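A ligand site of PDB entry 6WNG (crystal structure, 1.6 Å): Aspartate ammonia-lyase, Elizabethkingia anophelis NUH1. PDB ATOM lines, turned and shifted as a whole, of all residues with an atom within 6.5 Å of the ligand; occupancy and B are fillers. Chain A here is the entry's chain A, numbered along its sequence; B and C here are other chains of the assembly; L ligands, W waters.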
ATOM      1  N   GLY A 326       9.525 -28.262   3.164  1.00  0.00           N
ATOM      2  CA  GLY A 326       8.297 -28.306   2.404  1.00  0.00           C
ATOM      3  C   GLY A 326       7.813 -26.962   1.909  1.00  0.00           C
ATOM      4  O   GLY A 326       7.247 -26.865   0.813  1.00  0.00           O
ATOM      5  N   SER A 327       8.024 -25.901   2.699  1.00  0.00           N
ATOM      6  CA  SER A 327       7.268 -24.677   2.437  1.00  0.00           C
ATOM      7  C   SER A 327       8.084 -23.420   2.718  1.00  0.00           C
ATOM      8  O   SER A 327       8.809 -23.340   3.716  1.00  0.00           O
ATOM      9  CB  SER A 327       5.988 -24.655   3.283  1.00  0.00           C
ATOM     10  OG  SER A 327       5.267 -23.460   3.034  1.00  0.00           O
ATOM     11  N   SER A 328       7.923 -22.422   1.843  1.00  0.00           N
ATOM     12  CA  SER A 328       8.510 -21.108   2.057  1.00  0.00           C
ATOM     13  C   SER A 328       7.789 -20.322   3.154  1.00  0.00           C
ATOM     14  O   SER A 328       8.332 -19.332   3.636  1.00  0.00           O
ATOM     15  CB  SER A 328       8.477 -20.305   0.758  1.00  0.00           C
ATOM     16  OG  SER A 328       7.142 -19.972   0.402  1.00  0.00           O
ATOM     17  N   ILE A 329       6.585 -20.760   3.541  1.00  0.00           N
ATOM     18  CA  ILE A 329       5.774 -20.037   4.499  1.00  0.00           C
ATOM     19  C   ILE A 329       5.387 -20.898   5.701  1.00  0.00           C
ATOM     20  O   ILE A 329       5.378 -20.413   6.833  1.00  0.00           O
ATOM     21  CB  ILE A 329       4.517 -19.431   3.818  1.00  0.00           C
ATOM     22  CG1 ILE A 329       3.686 -18.615   4.818  1.00  0.00           C
ATOM     23  CG2 ILE A 329       3.678 -20.498   3.123  1.00  0.00           C
ATOM     24  CD1 ILE A 329       2.522 -17.860   4.177  1.00  0.00           C
ATOM     25  N   MET A 330       5.090 -22.190   5.497  1.00  0.00           N
ATOM     26  CA  MET A 330       4.604 -23.020   6.588  1.00  0.00           C
ATOM     27  C   MET A 330       5.769 -23.696   7.309  1.00  0.00           C
ATOM     28  O   MET A 330       6.353 -24.638   6.759  1.00  0.00           O
ATOM     29  CB  MET A 330       3.601 -24.041   6.074  1.00  0.00           C
ATOM     30  CG  MET A 330       2.263 -23.388   5.689  1.00  0.00           C
ATOM     31  SD  MET A 330       1.088 -24.415   4.776  1.00  0.00           S
ATOM     32  CE  MET A 330       1.802 -24.408   3.131  1.00  0.00           C
ATOM     33  N   LYS A 333       6.845 -27.888   7.832  1.00  0.00           N
ATOM     34  CA  LYS A 333       6.184 -28.740   6.846  1.00  0.00           C
ATOM     35  C   LYS A 333       7.208 -29.422   5.946  1.00  0.00           C
ATOM     36  O   LYS A 333       8.191 -28.816   5.534  1.00  0.00           O
ATOM     37  CB  LYS A 333       5.219 -27.881   6.030  1.00  0.00           C
ATOM     38  CG  LYS A 333       4.215 -28.630   5.169  1.00  0.00           C
ATOM     39  CD  LYS A 333       3.222 -27.597   4.581  1.00  0.00           C
ATOM     40  CE  LYS A 333       1.997 -28.246   3.978  1.00  0.00           C
ATOM     41  NZ  LYS A 333       2.271 -28.883   2.646  1.00  0.00           N
ATOM     42  N   ASN A 335       7.139 -32.260   2.571  1.00  0.00           N
ATOM     43  CA  ASN A 335       6.211 -32.818   1.604  1.00  0.00           C
ATOM     44  C   ASN A 335       6.776 -34.049   0.916  1.00  0.00           C
ATOM     45  O   ASN A 335       7.996 -34.249   0.867  1.00  0.00           O
ATOM     46  CB  ASN A 335       5.867 -31.750   0.564  1.00  0.00           C
ATOM     47  CG  ASN A 335       5.136 -30.582   1.185  1.00  0.00           C
ATOM     48  OD1 ASN A 335       4.310 -30.789   2.080  1.00  0.00           O
ATOM     49  ND2 ASN A 335       5.454 -29.377   0.763  1.00  0.00           N
ATOM     50  N   THR B 196      -2.043 -29.138   1.856  1.00  0.00           N
ATOM     51  CA  THR B 196      -1.384 -29.087   0.565  1.00  0.00           C
ATOM     52  C   THR B 196      -0.374 -30.231   0.509  1.00  0.00           C
ATOM     53  O   THR B 196       0.324 -30.509   1.494  1.00  0.00           O
ATOM     54  CB  THR B 196      -0.675 -27.743   0.311  1.00  0.00           C
ATOM     55  OG1 THR B 196       0.320 -27.523   1.315  1.00  0.00           O
ATOM     56  CG2 THR B 196      -1.706 -26.585   0.329  1.00  0.00           C
ATOM     57  N   GLN B 197      -0.302 -30.888  -0.655  1.00  0.00           N
ATOM     58  CA  GLN B 197       0.558 -32.059  -0.815  1.00  0.00           C
ATOM     59  C   GLN B 197       0.179 -33.161   0.170  1.00  0.00           C
ATOM     60  O   GLN B 197       0.998 -34.021   0.510  1.00  0.00           O
ATOM     61  CB  GLN B 197       2.050 -31.661  -0.733  1.00  0.00           C
ATOM     62  CG  GLN B 197       2.244 -30.215  -1.282  1.00  0.00           C
ATOM     63  CD  GLN B 197       3.608 -29.852  -1.849  1.00  0.00           C
ATOM     64  OE1 GLN B 197       3.935 -28.655  -1.963  1.00  0.00           O
ATOM     65  NE2 GLN B 197       4.394 -30.859  -2.220  1.00  0.00           N
ATOM     66  N   GLN B 199      -0.194 -32.810   3.207  1.00  0.00           N
ATOM     67  CA  GLN B 199       0.339 -32.475   4.526  1.00  0.00           C
ATOM     68  C   GLN B 199      -0.477 -31.350   5.156  1.00  0.00           C
ATOM     69  O   GLN B 199      -1.069 -30.519   4.446  1.00  0.00           O
ATOM     70  CB  GLN B 199       1.804 -32.077   4.427  1.00  0.00           C
ATOM     71  CG  GLN B 199       2.714 -33.211   3.927  1.00  0.00           C
ATOM     72  CD  GLN B 199       2.892 -34.316   4.947  1.00  0.00           C
ATOM     73  OE1 GLN B 199       3.380 -34.087   6.049  1.00  0.00           O
ATOM     74  NE2 GLN B 199       2.505 -35.537   4.574  1.00  0.00           N
ATOM     75  N   ALA B 201      -1.675 -28.029   6.371  1.00  0.00           N
ATOM     76  CA  ALA B 201      -1.309 -26.680   5.936  1.00  0.00           C
ATOM     77  C   ALA B 201      -1.684 -25.644   6.996  1.00  0.00           C
ATOM     78  O   ALA B 201      -1.001 -25.511   8.015  1.00  0.00           O
ATOM     79  CB  ALA B 201      -1.945 -26.365   4.584  1.00  0.00           C
ATOM     80  N   GLY C 107       7.787 -31.195  -5.099  1.00  0.00           N
ATOM     81  CA  GLY C 107       7.649 -30.022  -4.256  1.00  0.00           C
ATOM     82  C   GLY C 107       6.704 -28.953  -4.764  1.00  0.00           C
ATOM     83  O   GLY C 107       6.570 -27.897  -4.112  1.00  0.00           O
ATOM     84  N   ALA C 108       6.048 -29.185  -5.909  1.00  0.00           N
ATOM     85  CA  ALA C 108       4.934 -28.373  -6.400  1.00  0.00           C
ATOM     86  C   ALA C 108       5.334 -26.956  -6.779  1.00  0.00           C
ATOM     87  O   ALA C 108       4.465 -26.078  -6.905  1.00  0.00           O
ATOM     88  CB  ALA C 108       3.790 -28.328  -5.387  1.00  0.00           C
ATOM     89  N   GLY C 109       6.630 -26.705  -7.003  1.00  0.00           N
ATOM     90  CA  GLY C 109       7.102 -25.371  -7.327  1.00  0.00           C
ATOM     91  C   GLY C 109       7.889 -24.710  -6.223  1.00  0.00           C
ATOM     92  O   GLY C 109       8.531 -23.680  -6.475  1.00  0.00           O
ATOM     93  N   THR C 110       7.851 -25.251  -4.999  1.00  0.00           N
ATOM     94  CA  THR C 110       8.566 -24.644  -3.884  1.00  0.00           C
ATOM     95  C   THR C 110      10.043 -24.457  -4.201  1.00  0.00           C
ATOM     96  O   THR C 110      10.642 -23.445  -3.836  1.00  0.00           O
ATOM     97  CB  THR C 110       8.375 -25.489  -2.630  1.00  0.00           C
ATOM     98  OG1 THR C 110       6.995 -25.459  -2.228  1.00  0.00           O
ATOM     99  CG2 THR C 110       9.252 -25.016  -1.455  1.00  0.00           C
ATOM    100  N   ASN C 113      10.350 -21.339  -6.375  1.00  0.00           N
ATOM    101  CA  ASN C 113      10.140 -20.152  -5.554  1.00  0.00           C
ATOM    102  C   ASN C 113      11.325 -19.878  -4.636  1.00  0.00           C
ATOM    103  O   ASN C 113      11.788 -18.739  -4.520  1.00  0.00           O
ATOM    104  CB  ASN C 113       8.850 -20.287  -4.747  1.00  0.00           C
ATOM    105  CG  ASN C 113       8.498 -19.027  -3.972  1.00  0.00           C
ATOM    106  OD1 ASN C 113       8.654 -17.907  -4.480  1.00  0.00           O
ATOM    107  ND2 ASN C 113       8.047 -19.198  -2.733  1.00  0.00           N
ATOM    108  N   MET C 114      11.834 -20.914  -3.962  1.00  0.00           N
ATOM    109  CA  MET C 114      12.952 -20.711  -3.059  1.00  0.00           C
ATOM    110  C   MET C 114      14.233 -20.379  -3.816  1.00  0.00           C
ATOM    111  O   MET C 114      15.084 -19.650  -3.302  1.00  0.00           O
ATOM    112  CB  MET C 114      13.149 -21.930  -2.150  1.00  0.00           C
ATOM    113  CG  MET C 114      12.125 -22.035  -1.023  1.00  0.00           C
ATOM    114  SD  MET C 114      11.929 -20.549  -0.016  1.00  0.00           S
ATOM    115  CE  MET C 114      13.617 -20.245   0.510  1.00  0.00           C
ATOM    116  N   ASN C 145      10.445 -13.351   0.391  1.00  0.00           N
ATOM    117  CA  ASN C 145       9.172 -14.070   0.323  1.00  0.00           C
ATOM    118  C   ASN C 145       8.100 -13.456   1.209  1.00  0.00           C
ATOM    119  O   ASN C 145       7.042 -14.065   1.401  1.00  0.00           O
ATOM    120  CB  ASN C 145       9.391 -15.539   0.718  1.00  0.00           C
ATOM    121  CG  ASN C 145       8.337 -16.474   0.136  1.00  0.00           C
ATOM    122  OD1 ASN C 145       8.232 -16.626  -1.086  1.00  0.00           O
ATOM    123  ND2 ASN C 145       7.548 -17.108   1.009  1.00  0.00           N
ATOM    124  N   GLN C 148       4.106 -13.844   1.069  1.00  0.00           N
ATOM    125  CA  GLN C 148       3.912 -14.738  -0.066  1.00  0.00           C
ATOM    126  C   GLN C 148       3.976 -16.197   0.336  1.00  0.00           C
ATOM    127  O   GLN C 148       4.468 -16.567   1.417  1.00  0.00           O
ATOM    128  CB  GLN C 148       4.964 -14.518  -1.163  1.00  0.00           C
ATOM    129  CG  GLN C 148       5.047 -13.127  -1.725  1.00  0.00           C
ATOM    130  CD  GLN C 148       6.425 -12.854  -2.277  1.00  0.00           C
ATOM    131  OE1 GLN C 148       6.833 -13.469  -3.272  1.00  0.00           O
ATOM    132  NE2 GLN C 148       7.176 -11.965  -1.620  1.00  0.00           N
ATOM    133  N   SER C 149       3.480 -17.036  -0.573  1.00  0.00           N
ATOM    134  CA  SER C 149       3.734 -18.470  -0.583  1.00  0.00           C
ATOM    135  C   SER C 149       4.258 -18.825  -1.970  1.00  0.00           C
ATOM    136  O   SER C 149       4.085 -18.067  -2.929  1.00  0.00           O
ATOM    137  CB  SER C 149       2.445 -19.266  -0.270  1.00  0.00           C
ATOM    138  OG  SER C 149       2.601 -20.681  -0.375  1.00  0.00           O
ATOM    139  N   THR C 150       4.879 -19.989  -2.081  1.00  0.00           N
ATOM    140  CA  THR C 150       4.996 -20.609  -3.400  1.00  0.00           C
ATOM    141  C   THR C 150       3.629 -20.648  -4.080  1.00  0.00           C
ATOM    142  O   THR C 150       3.520 -20.484  -5.297  1.00  0.00           O
ATOM    143  CB  THR C 150       5.562 -22.027  -3.262  1.00  0.00           C
ATOM    144  OG1 THR C 150       6.859 -21.957  -2.669  1.00  0.00           O
ATOM    145  CG2 THR C 150       5.634 -22.722  -4.615  1.00  0.00           C
ATOM    146  N   ASN C 151       2.568 -20.854  -3.298  1.00  0.00           N
ATOM    147  CA  ASN C 151       1.289 -21.195  -3.899  1.00  0.00           C
ATOM    148  C   ASN C 151       0.557 -19.985  -4.449  1.00  0.00           C
ATOM    149  O   ASN C 151      -0.516 -20.163  -5.057  1.00  0.00           O
ATOM    150  CB  ASN C 151       0.446 -21.947  -2.859  1.00  0.00           C
ATOM    151  CG  ASN C 151       1.151 -23.209  -2.365  1.00  0.00           C
ATOM    152  OD1 ASN C 151       2.081 -23.698  -3.016  1.00  0.00           O
ATOM    153  ND2 ASN C 151       0.718 -23.730  -1.213  1.00  0.00           N
ATOM    154  N   THR C 239      -1.522 -16.451  -0.288  1.00  0.00           N
ATOM    155  CA  THR C 239      -0.515 -17.139   0.512  1.00  0.00           C
ATOM    156  C   THR C 239      -0.743 -18.644   0.450  1.00  0.00           C
ATOM    157  O   THR C 239      -0.860 -19.178  -0.661  1.00  0.00           O
ATOM    158  CB  THR C 239      -0.423 -16.545   1.951  1.00  0.00           C
ATOM    159  OG1 THR C 239      -1.527 -16.934   2.778  1.00  0.00           O
ATOM    160  CG2 THR C 239      -0.342 -15.017   1.898  1.00  0.00           C
ATOM    161  N   ALA C 240      -0.786 -19.352   1.586  1.00  0.00           N
ATOM    162  CA  ALA C 240      -0.599 -20.811   1.572  1.00  0.00           C
ATOM    163  C   ALA C 240      -1.727 -21.543   0.827  1.00  0.00           C
ATOM    164  O   ALA C 240      -1.464 -22.459   0.033  1.00  0.00           O
ATOM    165  CB  ALA C 240      -0.471 -21.342   3.002  1.00  0.00           C
ATOM    166  N   ILE C 241      -2.987 -21.214   1.105  1.00  0.00           N
ATOM    167  CA  ILE C 241      -4.106 -21.970   0.562  1.00  0.00           C
ATOM    168  C   ILE C 241      -5.214 -21.099  -0.011  1.00  0.00           C
ATOM    169  O   ILE C 241      -6.213 -21.635  -0.495  1.00  0.00           O
ATOM    170  CB  ILE C 241      -4.705 -22.939   1.596  1.00  0.00           C
ATOM    171  CG1 ILE C 241      -5.297 -22.174   2.784  1.00  0.00           C
ATOM    172  CG2 ILE C 241      -3.666 -23.959   2.074  1.00  0.00           C
ATOM    173  CD1 ILE C 241      -6.080 -23.064   3.768  1.00  0.00           C
ATOM    174  N   LEU C 367      -4.205 -27.779  -3.144  1.00  0.00           N
ATOM    175  CA  LEU C 367      -3.118 -27.532  -4.090  1.00  0.00           C
ATOM    176  C   LEU C 367      -3.036 -28.651  -5.120  1.00  0.00           C
ATOM    177  O   LEU C 367      -3.301 -29.822  -4.818  1.00  0.00           O
ATOM    178  CB  LEU C 367      -1.766 -27.433  -3.359  1.00  0.00           C
ATOM    179  CG  LEU C 367      -0.630 -26.822  -4.185  1.00  0.00           C
ATOM    180  CD1 LEU C 367      -0.936 -25.360  -4.487  1.00  0.00           C
ATOM    181  CD2 LEU C 367       0.703 -26.951  -3.460  1.00  0.00           C
HETATM  182  O1  LIG L   1       6.327 -23.313  -0.419  1.00  0.00           O
HETATM  183  C1  LIG L   1       5.245 -22.881  -0.041  1.00  0.00           C
HETATM  184  O2  LIG L   1       5.036 -21.692   0.219  1.00  0.00           O
HETATM  185  C2  LIG L   1       4.111 -23.840   0.084  1.00  0.00           C
HETATM  186  C3  LIG L   1       4.287 -25.163   0.173  1.00  0.00           C
HETATM  187  C4  LIG L   1       3.241 -26.172   0.473  1.00  0.00           C
HETATM  188  O3  LIG L   1       2.077 -25.906   0.166  1.00  0.00           O
HETATM  189  O4  LIG L   1       3.566 -27.180   1.080  1.00  0.00           O
HETATM  190  O   HOH W   1       4.156 -25.834  -2.993  1.00  0.00           O
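OG1 of Thr 196 of chain B lies within hydrogen-bond range of O3 of the ligand (2.6 Å).
O4 of the ligand is in salt-bridge range of NZ of Lys 333 (2.7 Å).
OG1 of Thr 150 of chain C is in hydrogen-bond range of O1 of the ligand (2.7 Å).
The backbone NH (N) of Thr 150 of chain C lies within hydrogen-bond range of an oxygen (O2) of the ligand, 2.9 Å away.
The side-chain amide nitrogen (ND2) of Asn 335 sits at hydrogen-bond distance from an oxygen (O4) of the ligand, at 2.9 Å.
The side-chain hydroxyl (OG) of Ser 327 lies close to an oxygen (O2) of the ligand (3.3 Å).
An oxygen (O2) of the ligand sits at hydrogen-bond distance from the side-chain hydroxyl (OG) of Ser 328 (2.7 Å).
O3 of the ligand is in hydrogen-bond range of ND2 of Asn 151 of chain C (2.9 Å).
OG of Ser 149 of chain C is in hydrogen-bond range of O2 of the ligand, 2.7 Å away.
The side-chain amide oxygen (OE1) of Gln 197 of chain B lies close to an oxygen (O4) of the ligand, 3.4 Å away.
An oxygen (O1) of the ligand lies within hydrogen-bond range of the side-chain hydroxyl of Thr 110 of chain C (2.9 Å).
N of Ser 328 is in hydrogen-bond range of O1 of the ligand (2.9 Å).
OG of Ser 327 is in hydrogen-bond range of N of Met 330, at 2.8 Å.
The side-chain amide nitrogen (ND2) of Asn 113 of chain C lies within hydrogen-bond range of the side-chain hydroxyl (OG1) of Thr 150 of chain C (3.0 Å).
The side-chain amide nitrogen of Asn 335 is in hydrogen-bond range of the side-chain amide oxygen of Gln 197 of chain B, at 3.2 Å.
The side-chain hydroxyl (OG) of Ser 149 of chain C sits at hydrogen-bond distance from the backbone NH (N) of Asn 151 of chain C (2.9 Å).
The side-chain amide nitrogen of Asn 113 of chain C lies within hydrogen-bond range of the side-chain hydroxyl of Ser 328, at 3.4 Å.
NZ of Lys 333 lies within hydrogen-bond range of OG1 of Thr 196 of chain B.
The backbone carbonyl oxygen (O) of Gly 107 of chain C sits at hydrogen-bond distance from the side-chain hydroxyl (OG1) of Thr 110 of chain C, at 3.1 Å.
The side-chain hydroxyl of Ser 328 sits at hydrogen-bond distance from the backbone NH of Thr 150 of chain C (3.4 Å).
Gly 326 touches the ligand.
Ile 329 touches the ligand (CG2 to O2, 3.4 Å).
Met 330 touches the ligand.
Hydrophobic or aromatic side chains that line the ligand: Ile 329 and Met 330.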
